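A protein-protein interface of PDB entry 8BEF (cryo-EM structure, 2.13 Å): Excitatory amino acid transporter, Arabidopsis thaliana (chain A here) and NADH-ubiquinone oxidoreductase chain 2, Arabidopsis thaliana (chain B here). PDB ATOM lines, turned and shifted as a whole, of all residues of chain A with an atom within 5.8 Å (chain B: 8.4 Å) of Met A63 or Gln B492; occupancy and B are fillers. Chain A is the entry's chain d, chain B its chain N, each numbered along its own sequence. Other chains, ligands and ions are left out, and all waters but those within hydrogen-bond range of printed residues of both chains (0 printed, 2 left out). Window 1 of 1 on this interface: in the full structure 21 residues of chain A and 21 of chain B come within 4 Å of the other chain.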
ATOM      1  N   LYS A  55     -36.482 -31.113  12.716  1.00  0.00           N
ATOM      2  CA  LYS A  55     -36.797 -30.552  11.404  1.00  0.00           C
ATOM      3  C   LYS A  55     -35.639 -29.712  10.866  1.00  0.00           C
ATOM      4  O   LYS A  55     -35.345 -29.739   9.662  1.00  0.00           O
ATOM      5  CB  LYS A  55     -38.101 -29.748  11.490  1.00  0.00           C
ATOM      6  CG  LYS A  55     -39.376 -30.539  11.762  1.00  0.00           C
ATOM      7  CD  LYS A  55     -40.616 -29.658  11.855  1.00  0.00           C
ATOM      8  CE  LYS A  55     -41.873 -30.490  12.104  1.00  0.00           C
ATOM      9  NZ  LYS A  55     -43.115 -29.679  12.228  1.00  0.00           N
ATOM     10  N   LEU A  56     -34.966 -28.966  11.748  1.00  0.00           N
ATOM     11  CA  LEU A  56     -33.827 -28.149  11.346  1.00  0.00           C
ATOM     12  C   LEU A  56     -32.695 -29.011  10.807  1.00  0.00           C
ATOM     13  O   LEU A  56     -32.071 -28.670   9.795  1.00  0.00           O
ATOM     14  CB  LEU A  56     -33.333 -27.320  12.532  1.00  0.00           C
ATOM     15  CG  LEU A  56     -34.063 -26.032  12.915  1.00  0.00           C
ATOM     16  CD1 LEU A  56     -33.519 -25.505  14.234  1.00  0.00           C
ATOM     17  CD2 LEU A  56     -33.939 -24.979  11.822  1.00  0.00           C
ATOM     18  N   GLU A  58     -33.084 -31.909   9.450  1.00  0.00           N
ATOM     19  CA  GLU A  58     -33.555 -32.424   8.165  1.00  0.00           C
ATOM     20  C   GLU A  58     -33.325 -31.423   7.036  1.00  0.00           C
ATOM     21  O   GLU A  58     -32.889 -31.801   5.943  1.00  0.00           O
ATOM     22  CB  GLU A  58     -35.034 -32.791   8.247  1.00  0.00           C
ATOM     23  CG  GLU A  58     -35.327 -34.045   9.041  1.00  0.00           C
ATOM     24  CD  GLU A  58     -36.518 -34.807   8.497  1.00  0.00           C
ATOM     25  OE1 GLU A  58     -36.476 -35.214   7.316  1.00  0.00           O
ATOM     26  OE2 GLU A  58     -37.497 -34.995   9.248  1.00  0.00           O
ATOM     27  N   ASP A  59     -33.618 -30.142   7.276  1.00  0.00           N
ATOM     28  CA  ASP A  59     -33.420 -29.149   6.219  1.00  0.00           C
ATOM     29  C   ASP A  59     -31.937 -28.900   5.955  1.00  0.00           C
ATOM     30  O   ASP A  59     -31.516 -28.772   4.792  1.00  0.00           O
ATOM     31  CB  ASP A  59     -34.128 -27.841   6.565  1.00  0.00           C
ATOM     32  CG  ASP A  59     -35.554 -28.054   7.014  1.00  0.00           C
ATOM     33  OD1 ASP A  59     -35.900 -27.590   8.116  1.00  0.00           O
ATOM     34  OD2 ASP A  59     -36.330 -28.690   6.271  1.00  0.00           O
ATOM     35  N   LEU A  60     -31.131 -28.826   7.020  1.00  0.00           N
ATOM     36  CA  LEU A  60     -29.696 -28.648   6.840  1.00  0.00           C
ATOM     37  C   LEU A  60     -29.088 -29.785   6.033  1.00  0.00           C
ATOM     38  O   LEU A  60     -28.133 -29.565   5.281  1.00  0.00           O
ATOM     39  CB  LEU A  60     -28.995 -28.530   8.192  1.00  0.00           C
ATOM     40  CG  LEU A  60     -27.491 -28.255   8.109  1.00  0.00           C
ATOM     41  CD1 LEU A  60     -27.215 -27.015   7.266  1.00  0.00           C
ATOM     42  CD2 LEU A  60     -26.874 -28.117   9.487  1.00  0.00           C
ATOM     43  N   ASP A  61     -29.625 -31.000   6.169  1.00  0.00           N
ATOM     44  CA  ASP A  61     -29.097 -32.125   5.400  1.00  0.00           C
ATOM     45  C   ASP A  61     -29.231 -31.887   3.900  1.00  0.00           C
ATOM     46  O   ASP A  61     -28.251 -31.995   3.154  1.00  0.00           O
ATOM     47  CB  ASP A  61     -29.809 -33.412   5.807  1.00  0.00           C
ATOM     48  CG  ASP A  61     -29.340 -33.928   7.147  1.00  0.00           C
ATOM     49  OD1 ASP A  61     -28.258 -33.501   7.595  1.00  0.00           O
ATOM     50  OD2 ASP A  61     -30.055 -34.751   7.756  1.00  0.00           O
ATOM     51  N   VAL A  62     -30.439 -31.551   3.444  1.00  0.00           N
ATOM     52  CA  VAL A  62     -30.660 -31.297   2.023  1.00  0.00           C
ATOM     53  C   VAL A  62     -29.811 -30.125   1.552  1.00  0.00           C
ATOM     54  O   VAL A  62     -29.279 -30.126   0.431  1.00  0.00           O
ATOM     55  CB  VAL A  62     -32.154 -31.044   1.749  1.00  0.00           C
ATOM     56  CG1 VAL A  62     -32.431 -31.095   0.259  1.00  0.00           C
ATOM     57  CG2 VAL A  62     -33.013 -32.041   2.507  1.00  0.00           C
ATOM     58  N   MET A  63     -29.681 -29.101   2.392  1.00  0.00           N
ATOM     59  CA  MET A  63     -28.977 -27.905   1.946  1.00  0.00           C
ATOM     60  C   MET A  63     -27.479 -28.176   1.801  1.00  0.00           C
ATOM     61  O   MET A  63     -26.847 -27.731   0.832  1.00  0.00           O
ATOM     62  CB  MET A  63     -29.260 -26.778   2.927  1.00  0.00           C
ATOM     63  CG  MET A  63     -30.062 -25.659   2.311  1.00  0.00           C
ATOM     64  SD  MET A  63     -30.309 -24.309   3.458  1.00  0.00           S
ATOM     65  CE  MET A  63     -28.866 -23.365   3.065  1.00  0.00           C
ATOM     66  N   LEU A  64     -26.905 -28.930   2.744  1.00  0.00           N
ATOM     67  CA  LEU A  64     -25.527 -29.390   2.605  1.00  0.00           C
ATOM     68  C   LEU A  64     -25.366 -30.299   1.395  1.00  0.00           C
ATOM     69  O   LEU A  64     -24.323 -30.283   0.738  1.00  0.00           O
ATOM     70  CB  LEU A  64     -25.084 -30.118   3.875  1.00  0.00           C
ATOM     71  CG  LEU A  64     -24.855 -29.293   5.141  1.00  0.00           C
ATOM     72  CD1 LEU A  64     -24.826 -30.186   6.361  1.00  0.00           C
ATOM     73  CD2 LEU A  64     -23.551 -28.532   5.020  1.00  0.00           C
ATOM     74  N   ALA A  65     -26.383 -31.109   1.093  1.00  0.00           N
ATOM     75  CA  ALA A  65     -26.316 -31.955  -0.095  1.00  0.00           C
ATOM     76  C   ALA A  65     -26.187 -31.111  -1.355  1.00  0.00           C
ATOM     77  O   ALA A  65     -25.370 -31.402  -2.238  1.00  0.00           O
ATOM     78  CB  ALA A  65     -27.552 -32.850  -0.177  1.00  0.00           C
ATOM     79  N   LYS A  66     -26.992 -30.052  -1.453  1.00  0.00           N
ATOM     80  CA  LYS A  66     -26.914 -29.178  -2.620  1.00  0.00           C
ATOM     81  C   LYS A  66     -25.572 -28.458  -2.685  1.00  0.00           C
ATOM     82  O   LYS A  66     -24.991 -28.314  -3.768  1.00  0.00           O
ATOM     83  CB  LYS A  66     -28.060 -28.171  -2.615  1.00  0.00           C
ATOM     84  CG  LYS A  66     -29.430 -28.795  -2.811  1.00  0.00           C
ATOM     85  CD  LYS A  66     -30.555 -27.767  -2.777  1.00  0.00           C
ATOM     86  CE  LYS A  66     -31.923 -28.391  -2.998  1.00  0.00           C
ATOM     87  NZ  LYS A  66     -32.999 -27.367  -2.935  1.00  0.00           N
ATOM     88  N   ALA A  67     -25.069 -27.992  -1.539  1.00  0.00           N
ATOM     89  CA  ALA A  67     -23.750 -27.365  -1.527  1.00  0.00           C
ATOM     90  C   ALA A  67     -22.678 -28.332  -2.019  1.00  0.00           C
ATOM     91  O   ALA A  67     -21.812 -27.957  -2.822  1.00  0.00           O
ATOM     92  CB  ALA A  67     -23.417 -26.862  -0.124  1.00  0.00           C
ATOM     93  N   ARG A  68     -22.728 -29.582  -1.553  1.00  0.00           N
ATOM     94  CA  ARG A  68     -21.754 -30.583  -1.976  1.00  0.00           C
ATOM     95  C   ARG A  68     -21.849 -30.857  -3.470  1.00  0.00           C
ATOM     96  O   ARG A  68     -20.826 -31.008  -4.142  1.00  0.00           O
ATOM     97  CB  ARG A  68     -21.953 -31.880  -1.193  1.00  0.00           C
ATOM     98  CG  ARG A  68     -20.930 -32.116  -0.098  1.00  0.00           C
ATOM     99  CD  ARG A  68     -21.400 -33.207   0.847  1.00  0.00           C
ATOM    100  NE  ARG A  68     -22.601 -32.812   1.575  1.00  0.00           N
ATOM    101  CZ  ARG A  68     -23.542 -33.654   1.980  1.00  0.00           C
ATOM    102  NH1 ARG A  68     -23.458 -34.952   1.739  1.00  0.00           N
ATOM    103  NH2 ARG A  68     -24.594 -33.182   2.640  1.00  0.00           N
ATOM    104  N   ASN B  91     -34.570 -17.785   3.123  1.00  0.00           N
ATOM    105  CA  ASN B  91     -34.464 -18.373   4.458  1.00  0.00           C
ATOM    106  C   ASN B  91     -33.671 -17.476   5.399  1.00  0.00           C
ATOM    107  O   ASN B  91     -34.038 -17.302   6.573  1.00  0.00           O
ATOM    108  CB  ASN B  91     -33.817 -19.757   4.367  1.00  0.00           C
ATOM    109  CG  ASN B  91     -34.740 -20.793   3.760  1.00  0.00           C
ATOM    110  OD1 ASN B  91     -35.946 -20.785   4.002  1.00  0.00           O
ATOM    111  ND2 ASN B  91     -34.175 -21.699   2.975  1.00  0.00           N
ATOM    112  N   PHE B  92     -32.579 -16.897   4.896  1.00  0.00           N
ATOM    113  CA  PHE B  92     -31.755 -16.007   5.703  1.00  0.00           C
ATOM    114  C   PHE B  92     -32.567 -14.820   6.210  1.00  0.00           C
ATOM    115  O   PHE B  92     -32.565 -14.516   7.412  1.00  0.00           O
ATOM    116  CB  PHE B  92     -30.551 -15.547   4.876  1.00  0.00           C
ATOM    117  CG  PHE B  92     -29.693 -14.526   5.559  1.00  0.00           C
ATOM    118  CD1 PHE B  92     -28.769 -14.906   6.515  1.00  0.00           C
ATOM    119  CD2 PHE B  92     -29.800 -13.186   5.235  1.00  0.00           C
ATOM    120  CE1 PHE B  92     -27.979 -13.968   7.146  1.00  0.00           C
ATOM    121  CE2 PHE B  92     -29.011 -12.245   5.860  1.00  0.00           C
ATOM    122  CZ  PHE B  92     -28.099 -12.636   6.815  1.00  0.00           C
ATOM    123  N   TYR B  94     -35.822 -14.648   6.367  1.00  0.00           N
ATOM    124  CA  TYR B  94     -36.830 -15.239   7.243  1.00  0.00           C
ATOM    125  C   TYR B  94     -36.368 -15.250   8.697  1.00  0.00           C
ATOM    126  O   TYR B  94     -36.999 -14.646   9.580  1.00  0.00           O
ATOM    127  CB  TYR B  94     -37.135 -16.653   6.746  1.00  0.00           C
ATOM    128  CG  TYR B  94     -38.083 -17.457   7.594  1.00  0.00           C
ATOM    129  CD1 TYR B  94     -39.450 -17.236   7.542  1.00  0.00           C
ATOM    130  CD2 TYR B  94     -37.610 -18.465   8.425  1.00  0.00           C
ATOM    131  CE1 TYR B  94     -40.320 -17.983   8.309  1.00  0.00           C
ATOM    132  CE2 TYR B  94     -38.470 -19.216   9.193  1.00  0.00           C
ATOM    133  CZ  TYR B  94     -39.823 -18.973   9.130  1.00  0.00           C
ATOM    134  OH  TYR B  94     -40.684 -19.715   9.898  1.00  0.00           O
ATOM    135  N   PHE B  95     -35.246 -15.926   8.960  1.00  0.00           N
ATOM    136  CA  PHE B  95     -34.782 -16.051  10.339  1.00  0.00           C
ATOM    137  C   PHE B  95     -34.333 -14.706  10.910  1.00  0.00           C
ATOM    138  O   PHE B  95     -34.583 -14.414  12.088  1.00  0.00           O
ATOM    139  CB  PHE B  95     -33.667 -17.093  10.426  1.00  0.00           C
ATOM    140  CG  PHE B  95     -34.149 -18.502  10.219  1.00  0.00           C
ATOM    141  CD1 PHE B  95     -35.072 -19.065  11.086  1.00  0.00           C
ATOM    142  CD2 PHE B  95     -33.692 -19.260   9.153  1.00  0.00           C
ATOM    143  CE1 PHE B  95     -35.526 -20.357  10.899  1.00  0.00           C
ATOM    144  CE2 PHE B  95     -34.143 -20.558   8.963  1.00  0.00           C
ATOM    145  CZ  PHE B  95     -35.060 -21.105   9.838  1.00  0.00           C
ATOM    146  N   ILE B 339     -17.814 -20.182   5.538  1.00  0.00           N
ATOM    147  CA  ILE B 339     -19.135 -20.616   6.068  1.00  0.00           C
ATOM    148  C   ILE B 339     -19.110 -20.641   7.625  1.00  0.00           C
ATOM    149  O   ILE B 339     -19.999 -20.098   8.190  1.00  0.00           O
ATOM    150  CB  ILE B 339     -19.649 -21.961   5.477  1.00  0.00           C
ATOM    151  CG1 ILE B 339     -19.985 -21.851   3.995  1.00  0.00           C
ATOM    152  CG2 ILE B 339     -20.851 -22.458   6.255  1.00  0.00           C
ATOM    153  CD1 ILE B 339     -21.001 -20.798   3.684  1.00  0.00           C
ATOM    154  N   ILE B 342     -19.256 -16.990   8.992  1.00  0.00           N
ATOM    155  CA  ILE B 342     -20.632 -16.417   8.951  1.00  0.00           C
ATOM    156  C   ILE B 342     -21.467 -17.034  10.080  1.00  0.00           C
ATOM    157  O   ILE B 342     -22.004 -16.282  10.845  1.00  0.00           O
ATOM    158  CB  ILE B 342     -21.320 -16.520   7.567  1.00  0.00           C
ATOM    159  CG1 ILE B 342     -20.763 -15.493   6.584  1.00  0.00           C
ATOM    160  CG2 ILE B 342     -22.816 -16.351   7.697  1.00  0.00           C
ATOM    161  CD1 ILE B 342     -19.335 -15.688   6.235  1.00  0.00           C
ATOM    162  N   GLN B 343     -21.383 -18.355  10.234  1.00  0.00           N
ATOM    163  CA  GLN B 343     -22.135 -19.030  11.284  1.00  0.00           C
ATOM    164  C   GLN B 343     -21.757 -18.500  12.659  1.00  0.00           C
ATOM    165  O   GLN B 343     -22.626 -18.257  13.504  1.00  0.00           O
ATOM    166  CB  GLN B 343     -21.899 -20.536  11.216  1.00  0.00           C
ATOM    167  CG  GLN B 343     -22.924 -21.347  11.968  1.00  0.00           C
ATOM    168  CD  GLN B 343     -22.448 -22.753  12.272  1.00  0.00           C
ATOM    169  OE1 GLN B 343     -21.318 -23.120  11.959  1.00  0.00           O
ATOM    170  NE2 GLN B 343     -23.309 -23.545  12.896  1.00  0.00           N
ATOM    171  N   LEU B 346     -23.212 -15.070  13.267  1.00  0.00           N
ATOM    172  CA  LEU B 346     -24.629 -15.148  13.616  1.00  0.00           C
ATOM    173  C   LEU B 346     -24.829 -15.635  15.049  1.00  0.00           C
ATOM    174  O   LEU B 346     -25.669 -15.098  15.784  1.00  0.00           O
ATOM    175  CB  LEU B 346     -25.359 -16.060  12.631  1.00  0.00           C
ATOM    176  CG  LEU B 346     -25.267 -15.668  11.154  1.00  0.00           C
ATOM    177  CD1 LEU B 346     -25.753 -16.794  10.244  1.00  0.00           C
ATOM    178  CD2 LEU B 346     -26.022 -14.378  10.883  1.00  0.00           C
ATOM    179  N   PRO B 485     -30.128 -26.495  18.251  1.00  0.00           N
ATOM    180  CA  PRO B 485     -30.995 -25.711  17.348  1.00  0.00           C
ATOM    181  C   PRO B 485     -30.353 -24.436  16.826  1.00  0.00           C
ATOM    182  O   PRO B 485     -30.485 -24.134  15.633  1.00  0.00           O
ATOM    183  CB  PRO B 485     -32.232 -25.410  18.208  1.00  0.00           C
ATOM    184  CG  PRO B 485     -32.189 -26.367  19.328  1.00  0.00           C
ATOM    185  CD  PRO B 485     -30.772 -26.745  19.555  1.00  0.00           C
ATOM    186  N   LEU B 486     -29.655 -23.682  17.680  1.00  0.00           N
ATOM    187  CA  LEU B 486     -28.973 -22.477  17.212  1.00  0.00           C
ATOM    188  C   LEU B 486     -27.896 -22.811  16.191  1.00  0.00           C
ATOM    189  O   LEU B 486     -27.770 -22.132  15.165  1.00  0.00           O
ATOM    190  CB  LEU B 486     -28.361 -21.715  18.388  1.00  0.00           C
ATOM    191  CG  LEU B 486     -27.830 -20.327  18.015  1.00  0.00           C
ATOM    192  CD1 LEU B 486     -28.907 -19.494  17.325  1.00  0.00           C
ATOM    193  CD2 LEU B 486     -27.254 -19.606  19.226  1.00  0.00           C
ATOM    194  N   PHE B 487     -27.105 -23.849  16.461  1.00  0.00           N
ATOM    195  CA  PHE B 487     -26.037 -24.232  15.545  1.00  0.00           C
ATOM    196  C   PHE B 487     -26.603 -24.607  14.182  1.00  0.00           C
ATOM    197  O   PHE B 487     -26.123 -24.137  13.142  1.00  0.00           O
ATOM    198  CB  PHE B 487     -25.243 -25.392  16.143  1.00  0.00           C
ATOM    199  CG  PHE B 487     -24.398 -25.005  17.322  1.00  0.00           C
ATOM    200  CD1 PHE B 487     -24.333 -23.687  17.748  1.00  0.00           C
ATOM    201  CD2 PHE B 487     -23.693 -25.965  18.025  1.00  0.00           C
ATOM    202  CE1 PHE B 487     -23.559 -23.332  18.835  1.00  0.00           C
ATOM    203  CE2 PHE B 487     -22.925 -25.615  19.115  1.00  0.00           C
ATOM    204  CZ  PHE B 487     -22.857 -24.296  19.518  1.00  0.00           C
ATOM    205  N   SER B 488     -27.657 -25.425  14.176  1.00  0.00           N
ATOM    206  CA  SER B 488     -28.260 -25.852  12.918  1.00  0.00           C
ATOM    207  C   SER B 488     -28.882 -24.682  12.168  1.00  0.00           C
ATOM    208  O   SER B 488     -28.702 -24.558  10.952  1.00  0.00           O
ATOM    209  CB  SER B 488     -29.302 -26.937  13.179  1.00  0.00           C
ATOM    210  OG  SER B 488     -28.761 -27.966  13.986  1.00  0.00           O
ATOM    211  N   VAL B 489     -29.608 -23.807  12.871  1.00  0.00           N
ATOM    212  CA  VAL B 489     -30.276 -22.705  12.186  1.00  0.00           C
ATOM    213  C   VAL B 489     -29.254 -21.713  11.635  1.00  0.00           C
ATOM    214  O   VAL B 489     -29.435 -21.166  10.541  1.00  0.00           O
ATOM    215  CB  VAL B 489     -31.311 -22.032  13.113  1.00  0.00           C
ATOM    216  CG1 VAL B 489     -30.644 -21.220  14.211  1.00  0.00           C
ATOM    217  CG2 VAL B 489     -32.257 -21.162  12.303  1.00  0.00           C
ATOM    218  N   THR B 490     -28.153 -21.488  12.358  1.00  0.00           N
ATOM    219  CA  THR B 490     -27.146 -20.550  11.873  1.00  0.00           C
ATOM    220  C   THR B 490     -26.369 -21.130  10.696  1.00  0.00           C
ATOM    221  O   THR B 490     -26.025 -20.400   9.759  1.00  0.00           O
ATOM    222  CB  THR B 490     -26.199 -20.147  13.003  1.00  0.00           C
ATOM    223  OG1 THR B 490     -25.834 -21.301  13.768  1.00  0.00           O
ATOM    224  CG2 THR B 490     -26.877 -19.128  13.918  1.00  0.00           C
ATOM    225  N   HIS B 491     -26.087 -22.437  10.720  1.00  0.00           N
ATOM    226  CA  HIS B 491     -25.482 -23.072   9.552  1.00  0.00           C
ATOM    227  C   HIS B 491     -26.408 -22.982   8.346  1.00  0.00           C
ATOM    228  O   HIS B 491     -25.965 -22.688   7.226  1.00  0.00           O
ATOM    229  CB  HIS B 491     -25.141 -24.529   9.864  1.00  0.00           C
ATOM    230  CG  HIS B 491     -24.073 -25.106   8.986  1.00  0.00           C
ATOM    231  ND1 HIS B 491     -23.191 -26.068   9.423  1.00  0.00           N
ATOM    232  CD2 HIS B 491     -23.752 -24.861   7.693  1.00  0.00           C
ATOM    233  CE1 HIS B 491     -22.368 -26.389   8.439  1.00  0.00           C
ATOM    234  NE2 HIS B 491     -22.689 -25.671   7.379  1.00  0.00           N
ATOM    235  N   GLN B 492     -27.702 -23.221   8.566  1.00  0.00           N
ATOM    236  CA  GLN B 492     -28.704 -23.063   7.521  1.00  0.00           C
ATOM    237  C   GLN B 492     -28.657 -21.667   6.913  1.00  0.00           C
ATOM    238  O   GLN B 492     -28.615 -21.512   5.690  1.00  0.00           O
ATOM    239  CB  GLN B 492     -30.087 -23.344   8.104  1.00  0.00           C
ATOM    240  CG  GLN B 492     -31.186 -23.525   7.095  1.00  0.00           C
ATOM    241  CD  GLN B 492     -32.420 -24.160   7.704  1.00  0.00           C
ATOM    242  OE1 GLN B 492     -32.325 -25.115   8.475  1.00  0.00           O
ATOM    243  NE2 GLN B 492     -33.587 -23.633   7.360  1.00  0.00           N
ATOM    244  N   MET B 493     -28.669 -20.637   7.759  1.00  0.00           N
ATOM    245  CA  MET B 493     -28.660 -19.262   7.262  1.00  0.00           C
ATOM    246  C   MET B 493     -27.381 -18.962   6.485  1.00  0.00           C
ATOM    247  O   MET B 493     -27.421 -18.395   5.379  1.00  0.00           O
ATOM    248  CB  MET B 493     -28.818 -18.293   8.434  1.00  0.00           C
ATOM    249  CG  MET B 493     -30.146 -18.408   9.155  1.00  0.00           C
ATOM    250  SD  MET B 493     -30.135 -17.565  10.744  1.00  0.00           S
ATOM    251  CE  MET B 493     -30.197 -15.861  10.203  1.00  0.00           C
ATOM    252  N   ALA B 494     -26.233 -19.373   7.009  1.00  0.00           N
ATOM    253  CA  ALA B 494     -24.924 -19.087   6.355  1.00  0.00           C
ATOM    254  C   ALA B 494     -24.947 -19.675   4.935  1.00  0.00           C
ATOM    255  O   ALA B 494     -24.592 -18.964   4.024  1.00  0.00           O
ATOM    256  CB  ALA B 494     -23.741 -19.582   7.135  1.00  0.00           C
ATOM    257  N   LEU B 495     -25.403 -20.898   4.813  1.00  0.00           N
ATOM    258  CA  LEU B 495     -25.544 -21.552   3.488  1.00  0.00           C
ATOM    259  C   LEU B 495     -26.523 -20.841   2.588  1.00  0.00           C
ATOM    260  O   LEU B 495     -26.180 -20.703   1.443  1.00  0.00           O
ATOM    261  CB  LEU B 495     -25.876 -23.035   3.655  1.00  0.00           C
ATOM    262  CG  LEU B 495     -24.710 -23.900   4.127  1.00  0.00           C
ATOM    263  CD1 LEU B 495     -25.170 -25.325   4.365  1.00  0.00           C
ATOM    264  CD2 LEU B 495     -23.575 -23.874   3.111  1.00  0.00           C
ATOM    265  N   SER B 496     -27.679 -20.390   3.094  1.00  0.00           N
ATOM    266  CA  SER B 496     -28.739 -19.757   2.274  1.00  0.00           C
ATOM    267  C   SER B 496     -28.284 -18.449   1.603  1.00  0.00           C
ATOM    268  O   SER B 496     -28.882 -18.123   0.606  1.00  0.00           O
ATOM    269  CB  SER B 496     -30.027 -19.573   3.099  1.00  0.00           C
ATOM    270  OG  SER B 496     -30.449 -20.780   3.700  1.00  0.00           O
ATOM    271  N   LEU B 497     -27.251 -17.775   2.106  1.00  0.00           N
ATOM    272  CA  LEU B 497     -26.665 -16.559   1.478  1.00  0.00           C
ATOM    273  C   LEU B 497     -26.219 -16.864   0.036  1.00  0.00           C
ATOM    274  O   LEU B 497     -26.465 -16.059  -0.801  1.00  0.00           O
ATOM    275  CB  LEU B 497     -25.479 -16.131   2.338  1.00  0.00           C
ATOM    276  CG  LEU B 497     -25.807 -15.323   3.591  1.00  0.00           C
ATOM    277  CD1 LEU B 497     -24.548 -15.008   4.382  1.00  0.00           C
ATOM    278  CD2 LEU B 497     -26.565 -14.049   3.253  1.00  0.00           C
ATOM    279  N   TYR B 498     -25.769 -18.074  -0.253  1.00  0.00           N
ATOM    280  CA  TYR B 498     -25.246 -18.433  -1.612  1.00  0.00           C
ATOM    281  C   TYR B 498     -26.000 -19.585  -2.241  1.00  0.00           C
ATOM    282  O   TYR B 498     -25.564 -20.038  -3.242  1.00  0.00           O
ATOM    283  CB  TYR B 498     -23.834 -18.959  -1.452  1.00  0.00           C
ATOM    284  CG  TYR B 498     -23.041 -18.258  -0.390  1.00  0.00           C
ATOM    285  CD1 TYR B 498     -23.053 -18.709   0.915  1.00  0.00           C
ATOM    286  CD2 TYR B 498     -22.327 -17.112  -0.685  1.00  0.00           C
ATOM    287  CE1 TYR B 498     -22.357 -18.043   1.906  1.00  0.00           C
ATOM    288  CE2 TYR B 498     -21.615 -16.443   0.290  1.00  0.00           C
ATOM    289  CZ  TYR B 498     -21.640 -16.907   1.590  1.00  0.00           C
ATOM    290  OH  TYR B 498     -20.954 -16.262   2.572  1.00  0.00           O
ATOM    291  N   LEU B 499     -27.032 -20.103  -1.604  1.00  0.00           N
ATOM    292  CA  LEU B 499     -27.711 -21.339  -2.052  1.00  0.00           C
ATOM    293  C   LEU B 499     -28.835 -21.678  -1.116  1.00  0.00           C
ATOM    294  O   LEU B 499     -29.869 -22.200  -1.605  1.00  0.00           O
ATOM    295  CB  LEU B 499     -26.675 -22.499  -1.982  1.00  0.00           C
ATOM    296  CG  LEU B 499     -26.339 -23.040  -0.595  1.00  0.00           C
ATOM    297  CD1 LEU B 499     -27.081 -24.336  -0.307  1.00  0.00           C
ATOM    298  CD2 LEU B 499     -24.841 -23.247  -0.453  1.00  0.00           C
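Leu A56 touches Pro B485.
Leu A56 touches Gln B492.
Gln B492 touches Asp A59.
CD1 of Leu B495 touches CD1 of Leu A60, 3.9 Å away.
Met A63 touches Gln B492 (CE to O, 3.2 Å).
Met A63 touches Leu B495.
CD1 of Leu B499 touches O of Met A63 (3.6 Å).
His B491 touches Leu A64 (NE2 to CD2, 3.8 Å).
Leu B495 touches Leu A64.
Leu B499 touches Ala A67.
The backbone carbonyl oxygen (O) of Lys A55 sits close to the side-chain carboxylate (OD1) of Asp A59, at 2.7 Å.
The backbone carbonyl oxygen of Leu A64 sits at hydrogen-bond distance from the guanidinium group of Arg A68 (3.2 Å).
The backbone carbonyl oxygen of Gln B492 sits at hydrogen-bond distance from the side-chain hydroxyl of Ser B496.
Of the printed residues of chain B, Leu A56 touches Pro B485 and Gln B492.
Glu A58 touches none of the printed residues of chain B.
Of the printed residues of chain B, Asp A59 touches Gln B492.
Of the printed residues of chain B, Met A63 touches Gln B492, Leu B495, Ser B496 and Leu B499.
Of chain A, only Leu A56, Asp A59 and Met A63 come within 4 Å of Gln B492.
Of the printed residues of chain A, Leu B495 touches Leu A60 (3.9 Å), Met A63 (3.1 Å) and Leu A64 (3.7 Å).
Printed residues of chain A within 4 Å of Leu B499: Met A63 and Ala A67.
Printed residues of chain A that touch a printed residue of chain B: Leu A56, Asp A59, Leu A60, Met A63, Leu A64 and Ala A67.
Hydrophobic or aromatic side chains of chain A within 4 Å of the printed part of chain B: Leu A56, Leu A60, Met A63, Leu A64 and Ala A67.
Hydrophobic or aromatic side chains of chain B that line the printed part of chain A: His B491, Leu B495 and Leu B499.
Among the printed residues, no Asp or Glu carboxylate lies within 4 Å of a Lys or Arg side-chain nitrogen of the other chain.
SD of Met A63 sits close to OG of Ser B496.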
